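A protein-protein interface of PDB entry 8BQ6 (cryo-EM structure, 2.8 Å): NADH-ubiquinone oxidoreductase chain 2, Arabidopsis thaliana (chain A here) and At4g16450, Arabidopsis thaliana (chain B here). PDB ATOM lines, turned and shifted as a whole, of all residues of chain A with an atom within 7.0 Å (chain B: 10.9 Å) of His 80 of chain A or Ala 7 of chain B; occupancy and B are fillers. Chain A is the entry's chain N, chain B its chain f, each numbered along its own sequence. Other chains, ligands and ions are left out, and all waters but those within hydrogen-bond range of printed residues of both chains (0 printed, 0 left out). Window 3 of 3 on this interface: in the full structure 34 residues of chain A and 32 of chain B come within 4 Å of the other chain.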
ATOM      1  N   ALA A  18       7.791  32.405  15.770  1.00  0.00           N
ATOM      2  CA  ALA A  18       7.133  31.935  14.561  1.00  0.00           C
ATOM      3  C   ALA A  18       7.704  32.562  13.295  1.00  0.00           C
ATOM      4  O   ALA A  18       7.450  32.047  12.201  1.00  0.00           O
ATOM      5  CB  ALA A  18       5.631  32.211  14.647  1.00  0.00           C
ATOM      6  N   PRO A  74       7.514  22.656  15.469  1.00  0.00           N
ATOM      7  CA  PRO A  74       6.373  23.057  16.311  1.00  0.00           C
ATOM      8  C   PRO A  74       6.378  24.528  16.676  1.00  0.00           C
ATOM      9  O   PRO A  74       5.318  25.092  16.976  1.00  0.00           O
ATOM     10  CB  PRO A  74       6.513  22.174  17.561  1.00  0.00           C
ATOM     11  CG  PRO A  74       7.668  21.277  17.322  1.00  0.00           C
ATOM     12  CD  PRO A  74       8.486  21.846  16.223  1.00  0.00           C
ATOM     13  N   LEU A  75       7.548  25.168  16.680  1.00  0.00           N
ATOM     14  CA  LEU A  75       7.614  26.560  17.103  1.00  0.00           C
ATOM     15  C   LEU A  75       7.089  27.506  16.034  1.00  0.00           C
ATOM     16  O   LEU A  75       6.744  28.652  16.341  1.00  0.00           O
ATOM     17  CB  LEU A  75       9.045  26.926  17.478  1.00  0.00           C
ATOM     18  CG  LEU A  75       9.670  26.067  18.573  1.00  0.00           C
ATOM     19  CD1 LEU A  75      11.086  26.521  18.809  1.00  0.00           C
ATOM     20  CD2 LEU A  75       8.862  26.160  19.853  1.00  0.00           C
ATOM     21  N   LEU A  76       7.017  27.053  14.782  1.00  0.00           N
ATOM     22  CA  LEU A  76       6.488  27.902  13.724  1.00  0.00           C
ATOM     23  C   LEU A  76       4.984  28.111  13.859  1.00  0.00           C
ATOM     24  O   LEU A  76       4.431  28.998  13.202  1.00  0.00           O
ATOM     25  CB  LEU A  76       6.821  27.302  12.358  1.00  0.00           C
ATOM     26  CG  LEU A  76       8.313  27.066  12.091  1.00  0.00           C
ATOM     27  CD1 LEU A  76       8.518  26.243  10.828  1.00  0.00           C
ATOM     28  CD2 LEU A  76       9.093  28.372  12.027  1.00  0.00           C
ATOM     29  N   THR A  77       4.314  27.319  14.695  1.00  0.00           N
ATOM     30  CA  THR A  77       2.890  27.479  14.953  1.00  0.00           C
ATOM     31  C   THR A  77       2.602  28.153  16.284  1.00  0.00           C
ATOM     32  O   THR A  77       1.448  28.165  16.720  1.00  0.00           O
ATOM     33  CB  THR A  77       2.184  26.124  14.915  1.00  0.00           C
ATOM     34  OG1 THR A  77       2.746  25.267  15.914  1.00  0.00           O
ATOM     35  CG2 THR A  77       2.357  25.484  13.559  1.00  0.00           C
ATOM     36  N   ILE A  78       3.621  28.695  16.949  1.00  0.00           N
ATOM     37  CA  ILE A  78       3.394  29.400  18.200  1.00  0.00           C
ATOM     38  C   ILE A  78       2.655  30.701  17.918  1.00  0.00           C
ATOM     39  O   ILE A  78       2.789  31.302  16.841  1.00  0.00           O
ATOM     40  CB  ILE A  78       4.724  29.658  18.932  1.00  0.00           C
ATOM     41  CG1 ILE A  78       4.560  29.431  20.429  1.00  0.00           C
ATOM     42  CG2 ILE A  78       5.201  31.085  18.722  1.00  0.00           C
ATOM     43  CD1 ILE A  78       5.861  29.493  21.173  1.00  0.00           C
ATOM     44  N   ALA A  79       1.851  31.131  18.891  1.00  0.00           N
ATOM     45  CA  ALA A  79       1.129  32.401  18.814  1.00  0.00           C
ATOM     46  C   ALA A  79       0.288  32.495  17.545  1.00  0.00           C
ATOM     47  O   ALA A  79       0.225  33.542  16.898  1.00  0.00           O
ATOM     48  CB  ALA A  79       2.094  33.584  18.911  1.00  0.00           C
ATOM     49  N   HIS A  80      -0.367  31.391  17.179  1.00  0.00           N
ATOM     50  CA  HIS A  80      -1.081  31.363  15.908  1.00  0.00           C
ATOM     51  C   HIS A  80      -2.268  32.319  15.894  1.00  0.00           C
ATOM     52  O   HIS A  80      -2.650  32.800  14.823  1.00  0.00           O
ATOM     53  CB  HIS A  80      -1.534  29.939  15.583  1.00  0.00           C
ATOM     54  CG  HIS A  80      -2.645  29.443  16.452  1.00  0.00           C
ATOM     55  ND1 HIS A  80      -2.555  29.395  17.826  1.00  0.00           N
ATOM     56  CD2 HIS A  80      -3.867  28.949  16.138  1.00  0.00           C
ATOM     57  CE1 HIS A  80      -3.677  28.908  18.322  1.00  0.00           C
ATOM     58  NE2 HIS A  80      -4.490  28.629  17.320  1.00  0.00           N
ATOM     59  N   LEU A  81      -2.865  32.609  17.053  1.00  0.00           N
ATOM     60  CA  LEU A  81      -3.976  33.559  17.079  1.00  0.00           C
ATOM     61  C   LEU A  81      -3.485  34.994  16.934  1.00  0.00           C
ATOM     62  O   LEU A  81      -4.123  35.808  16.258  1.00  0.00           O
ATOM     63  CB  LEU A  81      -4.787  33.409  18.364  1.00  0.00           C
ATOM     64  CG  LEU A  81      -5.460  32.072  18.666  1.00  0.00           C
ATOM     65  CD1 LEU A  81      -6.328  32.212  19.906  1.00  0.00           C
ATOM     66  CD2 LEU A  81      -6.282  31.594  17.480  1.00  0.00           C
ATOM     67  N   PHE A  82      -2.375  35.336  17.581  1.00  0.00           N
ATOM     68  CA  PHE A  82      -1.796  36.697  17.434  1.00  0.00           C
ATOM     69  C   PHE A  82      -1.374  36.915  15.979  1.00  0.00           C
ATOM     70  O   PHE A  82      -1.641  38.001  15.446  1.00  0.00           O
ATOM     71  CB  PHE A  82      -0.642  36.873  18.422  1.00  0.00           C
ATOM     72  CG  PHE A  82       0.216  38.097  18.222  1.00  0.00           C
ATOM     73  CD1 PHE A  82      -0.134  39.307  18.797  1.00  0.00           C
ATOM     74  CD2 PHE A  82       1.382  38.037  17.475  1.00  0.00           C
ATOM     75  CE1 PHE A  82       0.657  40.431  18.621  1.00  0.00           C
ATOM     76  CE2 PHE A  82       2.166  39.165  17.289  1.00  0.00           C
ATOM     77  CZ  PHE A  82       1.804  40.359  17.867  1.00  0.00           C
ATOM     78  N   TRP A  83      -0.767  35.909  15.354  1.00  0.00           N
ATOM     79  CA  TRP A  83      -0.274  36.025  13.991  1.00  0.00           C
ATOM     80  C   TRP A  83      -1.341  35.713  12.951  1.00  0.00           C
ATOM     81  O   TRP A  83      -1.033  35.705  11.757  1.00  0.00           O
ATOM     82  CB  TRP A  83       0.914  35.082  13.784  1.00  0.00           C
ATOM     83  CG  TRP A  83       2.167  35.471  14.511  1.00  0.00           C
ATOM     84  CD1 TRP A  83       2.782  34.763  15.496  1.00  0.00           C
ATOM     85  CD2 TRP A  83       2.974  36.633  14.289  1.00  0.00           C
ATOM     86  NE1 TRP A  83       3.910  35.415  15.917  1.00  0.00           N
ATOM     87  CE2 TRP A  83       4.053  36.566  15.190  1.00  0.00           C
ATOM     88  CE3 TRP A  83       2.885  37.726  13.425  1.00  0.00           C
ATOM     89  CZ2 TRP A  83       5.035  37.547  15.250  1.00  0.00           C
ATOM     90  CZ3 TRP A  83       3.864  38.699  13.487  1.00  0.00           C
ATOM     91  CH2 TRP A  83       4.923  38.603  14.393  1.00  0.00           C
ATOM     92  N   ASN A  84      -2.579  35.449  13.375  1.00  0.00           N
ATOM     93  CA  ASN A  84      -3.572  34.892  12.462  1.00  0.00           C
ATOM     94  C   ASN A  84      -3.940  35.872  11.355  1.00  0.00           C
ATOM     95  O   ASN A  84      -4.063  35.484  10.189  1.00  0.00           O
ATOM     96  CB  ASN A  84      -4.812  34.460  13.243  1.00  0.00           C
ATOM     97  CG  ASN A  84      -5.974  34.116  12.345  1.00  0.00           C
ATOM     98  OD1 ASN A  84      -5.904  33.172  11.561  1.00  0.00           O
ATOM     99  ND2 ASN A  84      -7.058  34.867  12.464  1.00  0.00           N
ATOM    100  N   ASN A  85      -4.103  37.148  11.687  1.00  0.00           N
ATOM    101  CA  ASN A  85      -4.450  38.133  10.671  1.00  0.00           C
ATOM    102  C   ASN A  85      -3.280  38.512   9.769  1.00  0.00           C
ATOM    103  O   ASN A  85      -3.468  39.332   8.865  1.00  0.00           O
ATOM    104  CB  ASN A  85      -5.049  39.379  11.330  1.00  0.00           C
ATOM    105  CG  ASN A  85      -6.435  39.122  11.889  1.00  0.00           C
ATOM    106  OD1 ASN A  85      -6.721  39.409  13.048  1.00  0.00           O
ATOM    107  ND2 ASN A  85      -7.306  38.582  11.052  1.00  0.00           N
ATOM    108  N   PHE A  87      -0.495  35.818   8.749  1.00  0.00           N
ATOM    109  CA  PHE A  87      -0.091  34.646   7.977  1.00  0.00           C
ATOM    110  C   PHE A  87      -0.537  33.396   8.728  1.00  0.00           C
ATOM    111  O   PHE A  87      -1.039  33.468   9.854  1.00  0.00           O
ATOM    112  CB  PHE A  87       1.418  34.622   7.729  1.00  0.00           C
ATOM    113  CG  PHE A  87       2.229  34.660   8.984  1.00  0.00           C
ATOM    114  CD1 PHE A  87       2.485  33.502   9.696  1.00  0.00           C
ATOM    115  CD2 PHE A  87       2.737  35.855   9.454  1.00  0.00           C
ATOM    116  CE1 PHE A  87       3.222  33.540  10.853  1.00  0.00           C
ATOM    117  CE2 PHE A  87       3.479  35.895  10.608  1.00  0.00           C
ATOM    118  CZ  PHE A  87       3.721  34.738  11.310  1.00  0.00           C
ATOM    119  N   ARG A  88      -0.310  32.240   8.103  1.00  0.00           N
ATOM    120  CA  ARG A  88      -0.721  30.949   8.642  1.00  0.00           C
ATOM    121  C   ARG A  88       0.349  29.913   8.337  1.00  0.00           C
ATOM    122  O   ARG A  88       0.580  29.583   7.171  1.00  0.00           O
ATOM    123  CB  ARG A  88      -2.067  30.518   8.053  1.00  0.00           C
ATOM    124  CG  ARG A  88      -2.636  29.253   8.656  1.00  0.00           C
ATOM    125  CD  ARG A  88      -2.953  29.482  10.116  1.00  0.00           C
ATOM    126  NE  ARG A  88      -4.245  30.116  10.374  1.00  0.00           N
ATOM    127  CZ  ARG A  88      -5.419  29.710   9.907  1.00  0.00           C
ATOM    128  NH1 ARG A  88      -5.549  28.576   9.235  1.00  0.00           N
ATOM    129  NH2 ARG A  88      -6.503  30.440  10.157  1.00  0.00           N
ATOM    130  N   ARG A  89       0.984  29.391   9.383  1.00  0.00           N
ATOM    131  CA  ARG A  89       2.036  28.392   9.257  1.00  0.00           C
ATOM    132  C   ARG A  89       1.504  27.039   9.705  1.00  0.00           C
ATOM    133  O   ARG A  89       0.950  26.920  10.803  1.00  0.00           O
ATOM    134  CB  ARG A  89       3.259  28.782  10.089  1.00  0.00           C
ATOM    135  CG  ARG A  89       3.913  30.069   9.637  1.00  0.00           C
ATOM    136  CD  ARG A  89       5.285  30.253  10.256  1.00  0.00           C
ATOM    137  NE  ARG A  89       6.326  29.791   9.347  1.00  0.00           N
ATOM    138  CZ  ARG A  89       7.422  30.474   9.046  1.00  0.00           C
ATOM    139  NH1 ARG A  89       7.663  31.663   9.572  1.00  0.00           N
ATOM    140  NH2 ARG A  89       8.295  29.950   8.190  1.00  0.00           N
ATOM    141  N   ASN B   2      -2.581  43.442  22.597  1.00  0.00           N
ATOM    142  CA  ASN B   2      -3.033  42.119  23.112  1.00  0.00           C
ATOM    143  C   ASN B   2      -2.212  41.002  22.472  1.00  0.00           C
ATOM    144  O   ASN B   2      -1.975  41.063  21.252  1.00  0.00           O
ATOM    145  CB  ASN B   2      -4.527  41.881  22.893  1.00  0.00           C
ATOM    146  CG  ASN B   2      -5.391  42.792  23.738  1.00  0.00           C
ATOM    147  OD1 ASN B   2      -6.182  43.567  23.211  1.00  0.00           O
ATOM    148  ND2 ASN B   2      -5.242  42.708  25.050  1.00  0.00           N
ATOM    149  N   THR B   3      -1.802  40.022  23.275  1.00  0.00           N
ATOM    150  CA  THR B   3      -0.931  38.934  22.768  1.00  0.00           C
ATOM    151  C   THR B   3      -1.483  37.572  23.187  1.00  0.00           C
ATOM    152  O   THR B   3      -2.348  37.531  24.087  1.00  0.00           O
ATOM    153  CB  THR B   3       0.498  39.096  23.297  1.00  0.00           C
ATOM    154  OG1 THR B   3       0.461  39.042  24.723  1.00  0.00           O
ATOM    155  CG2 THR B   3       1.168  40.380  22.860  1.00  0.00           C
ATOM    156  N   ASP B   4      -0.975  36.501  22.583  1.00  0.00           N
ATOM    157  CA  ASP B   4      -1.406  35.154  22.934  1.00  0.00           C
ATOM    158  C   ASP B   4      -0.353  34.183  22.423  1.00  0.00           C
ATOM    159  O   ASP B   4      -0.212  34.008  21.210  1.00  0.00           O
ATOM    160  CB  ASP B   4      -2.776  34.859  22.346  1.00  0.00           C
ATOM    161  CG  ASP B   4      -3.523  33.823  23.137  1.00  0.00           C
ATOM    162  OD1 ASP B   4      -3.364  32.629  22.827  1.00  0.00           O
ATOM    163  OD2 ASP B   4      -4.253  34.192  24.078  1.00  0.00           O
ATOM    164  N   ILE B   5       0.383  33.562  23.349  1.00  0.00           N
ATOM    165  CA  ILE B   5       1.451  32.640  22.983  1.00  0.00           C
ATOM    166  C   ILE B   5       0.932  31.290  22.510  1.00  0.00           C
ATOM    167  O   ILE B   5       1.700  30.518  21.927  1.00  0.00           O
ATOM    168  CB  ILE B   5       2.413  32.461  24.178  1.00  0.00           C
ATOM    169  CG1 ILE B   5       3.798  31.992  23.717  1.00  0.00           C
ATOM    170  CG2 ILE B   5       1.834  31.497  25.199  1.00  0.00           C
ATOM    171  CD1 ILE B   5       4.521  32.972  22.838  1.00  0.00           C
ATOM    172  N   THR B   6      -0.354  31.001  22.720  1.00  0.00           N
ATOM    173  CA  THR B   6      -0.902  29.666  22.494  1.00  0.00           C
ATOM    174  C   THR B   6      -0.596  29.163  21.094  1.00  0.00           C
ATOM    175  O   THR B   6      -0.893  29.830  20.098  1.00  0.00           O
ATOM    176  CB  THR B   6      -2.414  29.673  22.728  1.00  0.00           C
ATOM    177  OG1 THR B   6      -2.682  29.723  24.133  1.00  0.00           O
ATOM    178  CG2 THR B   6      -3.063  28.430  22.133  1.00  0.00           C
ATOM    179  N   ALA B   7      -0.013  27.977  21.025  1.00  0.00           N
ATOM    180  CA  ALA B   7       0.376  27.396  19.755  1.00  0.00           C
ATOM    181  C   ALA B   7      -0.746  26.532  19.199  1.00  0.00           C
ATOM    182  O   ALA B   7      -1.643  26.085  19.917  1.00  0.00           O
ATOM    183  CB  ALA B   7       1.652  26.572  19.909  1.00  0.00           C
ATOM    184  N   LEU B   8      -0.688  26.321  17.885  1.00  0.00           N
ATOM    185  CA  LEU B   8      -1.657  25.471  17.207  1.00  0.00           C
ATOM    186  C   LEU B   8      -1.531  24.023  17.658  1.00  0.00           C
ATOM    187  O   LEU B   8      -2.535  23.329  17.857  1.00  0.00           O
ATOM    188  CB  LEU B   8      -1.448  25.576  15.702  1.00  0.00           C
ATOM    189  CG  LEU B   8      -2.356  24.749  14.805  1.00  0.00           C
ATOM    190  CD1 LEU B   8      -3.814  25.036  15.119  1.00  0.00           C
ATOM    191  CD2 LEU B   8      -2.022  25.022  13.357  1.00  0.00           C
ATOM    192  N   GLU B   9      -0.302  23.546  17.805  1.00  0.00           N
ATOM    193  CA  GLU B   9      -0.024  22.178  18.208  1.00  0.00           C
ATOM    194  C   GLU B   9       0.506  22.182  19.634  1.00  0.00           C
ATOM    195  O   GLU B   9       1.504  22.847  19.928  1.00  0.00           O
ATOM    196  CB  GLU B   9       0.971  21.529  17.252  1.00  0.00           C
ATOM    197  CG  GLU B   9       0.361  21.250  15.900  1.00  0.00           C
ATOM    198  CD  GLU B   9      -0.597  20.084  15.959  1.00  0.00           C
ATOM    199  OE1 GLU B   9      -0.168  19.001  16.406  1.00  0.00           O
ATOM    200  OE2 GLU B   9      -1.777  20.249  15.581  1.00  0.00           O
ATOM    201  N   LYS B  10      -0.160  21.438  20.508  1.00  0.00           N
ATOM    202  CA  LYS B  10       0.149  21.506  21.923  1.00  0.00           C
ATOM    203  C   LYS B  10       1.496  20.860  22.226  1.00  0.00           C
ATOM    204  O   LYS B  10       1.918  19.889  21.589  1.00  0.00           O
ATOM    205  CB  LYS B  10      -0.954  20.842  22.745  1.00  0.00           C
ATOM    206  CG  LYS B  10      -2.350  21.435  22.534  1.00  0.00           C
ATOM    207  CD  LYS B  10      -2.398  22.973  22.458  1.00  0.00           C
ATOM    208  CE  LYS B  10      -1.735  23.672  23.646  1.00  0.00           C
ATOM    209  NZ  LYS B  10      -2.541  24.823  24.135  1.00  0.00           N
ATOM    210  N   ALA B  11       2.172  21.430  23.219  1.00  0.00           N
ATOM    211  CA  ALA B  11       3.435  20.891  23.697  1.00  0.00           C
ATOM    212  C   ALA B  11       3.255  19.463  24.189  1.00  0.00           C
ATOM    213  O   ALA B  11       2.343  19.164  24.965  1.00  0.00           O
ATOM    214  CB  ALA B  11       3.986  21.763  24.821  1.00  0.00           C
ATOM    215  N   GLN B  12       4.145  18.582  23.740  1.00  0.00           N
ATOM    216  CA  GLN B  12       4.093  17.160  24.046  1.00  0.00           C
ATOM    217  C   GLN B  12       4.938  16.778  25.247  1.00  0.00           C
ATOM    218  O   GLN B  12       5.144  15.587  25.492  1.00  0.00           O
ATOM    219  CB  GLN B  12       4.556  16.350  22.844  1.00  0.00           C
ATOM    220  CG  GLN B  12       3.463  15.669  22.087  1.00  0.00           C
ATOM    221  CD  GLN B  12       3.907  15.343  20.689  1.00  0.00           C
ATOM    222  OE1 GLN B  12       5.068  15.006  20.465  1.00  0.00           O
ATOM    223  NE2 GLN B  12       2.990  15.439  19.736  1.00  0.00           N
ATOM    224  N   VAL B  15       5.311  21.257  30.532  1.00  0.00           N
ATOM    225  CA  VAL B  15       5.467  22.681  30.271  1.00  0.00           C
ATOM    226  C   VAL B  15       6.088  23.291  31.523  1.00  0.00           C
ATOM    227  O   VAL B  15       5.409  23.529  32.523  1.00  0.00           O
ATOM    228  CB  VAL B  15       4.135  23.338  29.902  1.00  0.00           C
ATOM    229  CG1 VAL B  15       4.242  24.848  29.976  1.00  0.00           C
ATOM    230  CG2 VAL B  15       3.708  22.902  28.514  1.00  0.00           C
ATOM    231  N   ARG B  18       5.399  28.584  30.426  1.00  0.00           N
ATOM    232  CA  ARG B  18       4.632  28.832  29.206  1.00  0.00           C
ATOM    233  C   ARG B  18       5.289  29.881  28.318  1.00  0.00           C
ATOM    234  O   ARG B  18       5.446  29.671  27.109  1.00  0.00           O
ATOM    235  CB  ARG B  18       3.212  29.274  29.559  1.00  0.00           C
ATOM    236  CG  ARG B  18       2.302  29.440  28.359  1.00  0.00           C
ATOM    237  CD  ARG B  18       0.880  29.785  28.767  1.00  0.00           C
ATOM    238  NE  ARG B  18       0.019  29.965  27.604  1.00  0.00           N
ATOM    239  CZ  ARG B  18      -0.574  28.979  26.943  1.00  0.00           C
ATOM    240  NH1 ARG B  18      -0.432  27.716  27.312  1.00  0.00           N
ATOM    241  NH2 ARG B  18      -1.325  29.268  25.885  1.00  0.00           N
ATOM    242  N   ASN B  19       5.649  31.026  28.891  1.00  0.00           N
ATOM    243  CA  ASN B  19       6.210  32.155  28.148  1.00  0.00           C
ATOM    244  C   ASN B  19       7.476  32.614  28.856  1.00  0.00           C
ATOM    245  O   ASN B  19       7.491  33.648  29.532  1.00  0.00           O
ATOM    246  CB  ASN B  19       5.191  33.293  28.046  1.00  0.00           C
ATOM    247  CG  ASN B  19       5.493  34.258  26.919  1.00  0.00           C
ATOM    248  OD1 ASN B  19       6.650  34.488  26.571  1.00  0.00           O
ATOM    249  ND2 ASN B  19       4.447  34.840  26.349  1.00  0.00           N
ATOM    250  N   ALA B  82      14.166  27.769  24.430  1.00  0.00           N
ATOM    251  CA  ALA B  82      12.790  28.180  24.672  1.00  0.00           C
ATOM    252  C   ALA B  82      11.818  27.048  24.372  1.00  0.00           C
ATOM    253  O   ALA B  82      10.820  26.877  25.080  1.00  0.00           O
ATOM    254  CB  ALA B  82      12.454  29.417  23.841  1.00  0.00           C
ATOM    255  N   GLY B  83      12.091  26.257  23.331  1.00  0.00           N
ATOM    256  CA  GLY B  83      11.250  25.104  23.069  1.00  0.00           C
ATOM    257  C   GLY B  83      11.287  24.089  24.195  1.00  0.00           C
ATOM    258  O   GLY B  83      10.275  23.459  24.509  1.00  0.00           O
ATOM    259  N   MET B  86       9.248  25.473  27.093  1.00  0.00           N
ATOM    260  CA  MET B  86       7.828  25.481  26.766  1.00  0.00           C
ATOM    261  C   MET B  86       7.239  24.089  26.566  1.00  0.00           C
ATOM    262  O   MET B  86       6.024  23.974  26.376  1.00  0.00           O
ATOM    263  CB  MET B  86       7.583  26.305  25.497  1.00  0.00           C
ATOM    264  CG  MET B  86       7.807  27.798  25.640  1.00  0.00           C
ATOM    265  SD  MET B  86       8.029  28.572  24.028  1.00  0.00           S
ATOM    266  CE  MET B  86       7.740  30.286  24.434  1.00  0.00           C
ATOM    267  N   GLY B  87       8.053  23.040  26.592  1.00  0.00           N
ATOM    268  CA  GLY B  87       7.559  21.691  26.416  1.00  0.00           C
ATOM    269  C   GLY B  87       7.421  21.217  24.988  1.00  0.00           C
ATOM    270  O   GLY B  87       6.829  20.155  24.764  1.00  0.00           O
ATOM    271  N   PHE B  88       7.944  21.962  24.013  1.00  0.00           N
ATOM    272  CA  PHE B  88       7.832  21.541  22.620  1.00  0.00           C
ATOM    273  C   PHE B  88       8.914  20.546  22.223  1.00  0.00           C
ATOM    274  O   PHE B  88       8.697  19.729  21.322  1.00  0.00           O
ATOM    275  CB  PHE B  88       7.878  22.757  21.700  1.00  0.00           C
ATOM    276  CG  PHE B  88       6.659  23.614  21.787  1.00  0.00           C
ATOM    277  CD1 PHE B  88       5.472  23.205  21.210  1.00  0.00           C
ATOM    278  CD2 PHE B  88       6.693  24.820  22.459  1.00  0.00           C
ATOM    279  CE1 PHE B  88       4.347  23.985  21.293  1.00  0.00           C
ATOM    280  CE2 PHE B  88       5.570  25.606  22.546  1.00  0.00           C
ATOM    281  CZ  PHE B  88       4.393  25.187  21.963  1.00  0.00           C
ATOM    282  N   PHE B  89      10.071  20.600  22.870  1.00  0.00           N
ATOM    283  CA  PHE B  89      11.182  19.690  22.653  1.00  0.00           C
ATOM    284  C   PHE B  89      11.413  18.872  23.914  1.00  0.00           C
ATOM    285  O   PHE B  89      11.071  19.311  25.016  1.00  0.00           O
ATOM    286  CB  PHE B  89      12.463  20.462  22.303  1.00  0.00           C
ATOM    287  CG  PHE B  89      12.319  21.365  21.124  1.00  0.00           C
ATOM    288  CD1 PHE B  89      11.711  20.922  19.967  1.00  0.00           C
ATOM    289  CD2 PHE B  89      12.774  22.668  21.178  1.00  0.00           C
ATOM    290  CE1 PHE B  89      11.572  21.754  18.882  1.00  0.00           C
ATOM    291  CE2 PHE B  89      12.632  23.508  20.097  1.00  0.00           C
ATOM    292  CZ  PHE B  89      12.031  23.049  18.946  1.00  0.00           C
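O of Thr 77 of chain A sits at hydrogen-bond distance from N of Leu 8 of chain B (3.1 Å).
The backbone carbonyl oxygen of Ile 5 of chain B sits at hydrogen-bond distance from the backbone NH of Ala 79 of chain A (3.1 Å).
The backbone NH of Ala 79 of chain A sits at hydrogen-bond distance from the backbone carbonyl oxygen of Thr 6 of chain B (3.3 Å).
ND1 of His 80 of chain A sits at hydrogen-bond distance from O of Thr 6 of chain B (2.8 Å).
OG1 of Thr 77 of chain A lies within hydrogen-bond range of O of Pro 74 of chain A (2.8 Å).
The side-chain carboxylate (OD1) of Asp 4 of chain B sits close to the side-chain hydroxyl (OG1) of Thr 6 of chain B (3.3 Å).
O of Gly 83 of chain B is in hydrogen-bond range of N of Phe 88 of chain B.
The backbone carbonyl oxygen (O) of Gly 83 of chain B sits at hydrogen-bond distance from the backbone NH (N) of Phe 89 of chain B (3.3 Å).
Among the printed residues, merely in contact across the chains: Pro 74 of chain A with Phe 88 of chain B, Leu 75 of chain A with Phe 88 of chain B, Leu 75 of chain A with Phe 89 of chain B, Thr 77 of chain A with Ala 7 of chain B, Thr 77 of chain A with Glu 9 of chain B, Ile 78 of chain A with Ile 5 of chain B, Ile 78 of chain A with Ala 7 of chain B, Ile 78 of chain A with Met 86 of chain B, Ala 79 of chain A with Asp 4 of chain B, His 80 of chain A with Ala 7 of chain B, His 80 of chain A with Leu 8 of chain B and Phe 82 of chain A with Asn 2 of chain B.
Of the printed residues of chain B, His 80 of chain A touches Thr 6, Ala 7 and Leu 8.
Printed residues of chain A within 4 Å of Ala 7 of chain B: Thr 77, Ile 78 and His 80.
Ile 78 of chain A touches three residues of chain B.
Of chain B, only Asp 4, Ile 5 and Thr 6 come within 4 Å of Ala 79 of chain A.
No residue of chain B comes within 4 Å of Leu 81 of chain A.
Of the printed residues of chain A, Glu 9 of chain B touches Thr 77.
Printed residues of chain A within 4 Å of Asn 2 of chain B: Phe 82.
Hydrophobic or aromatic side chains of chain A within 4 Å of the printed part of chain B: Pro 74, Leu 75, Ile 78, Ala 79, His 80 and Phe 82.
Along chain A the printed residues that touch a printed residue of chain B span positions 74 to 82.
Hydrophobic or aromatic side chains of chain B within 4 Å of the printed part of chain A: Ala 7, Leu 8, Met 86, Phe 88 and Phe 89.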
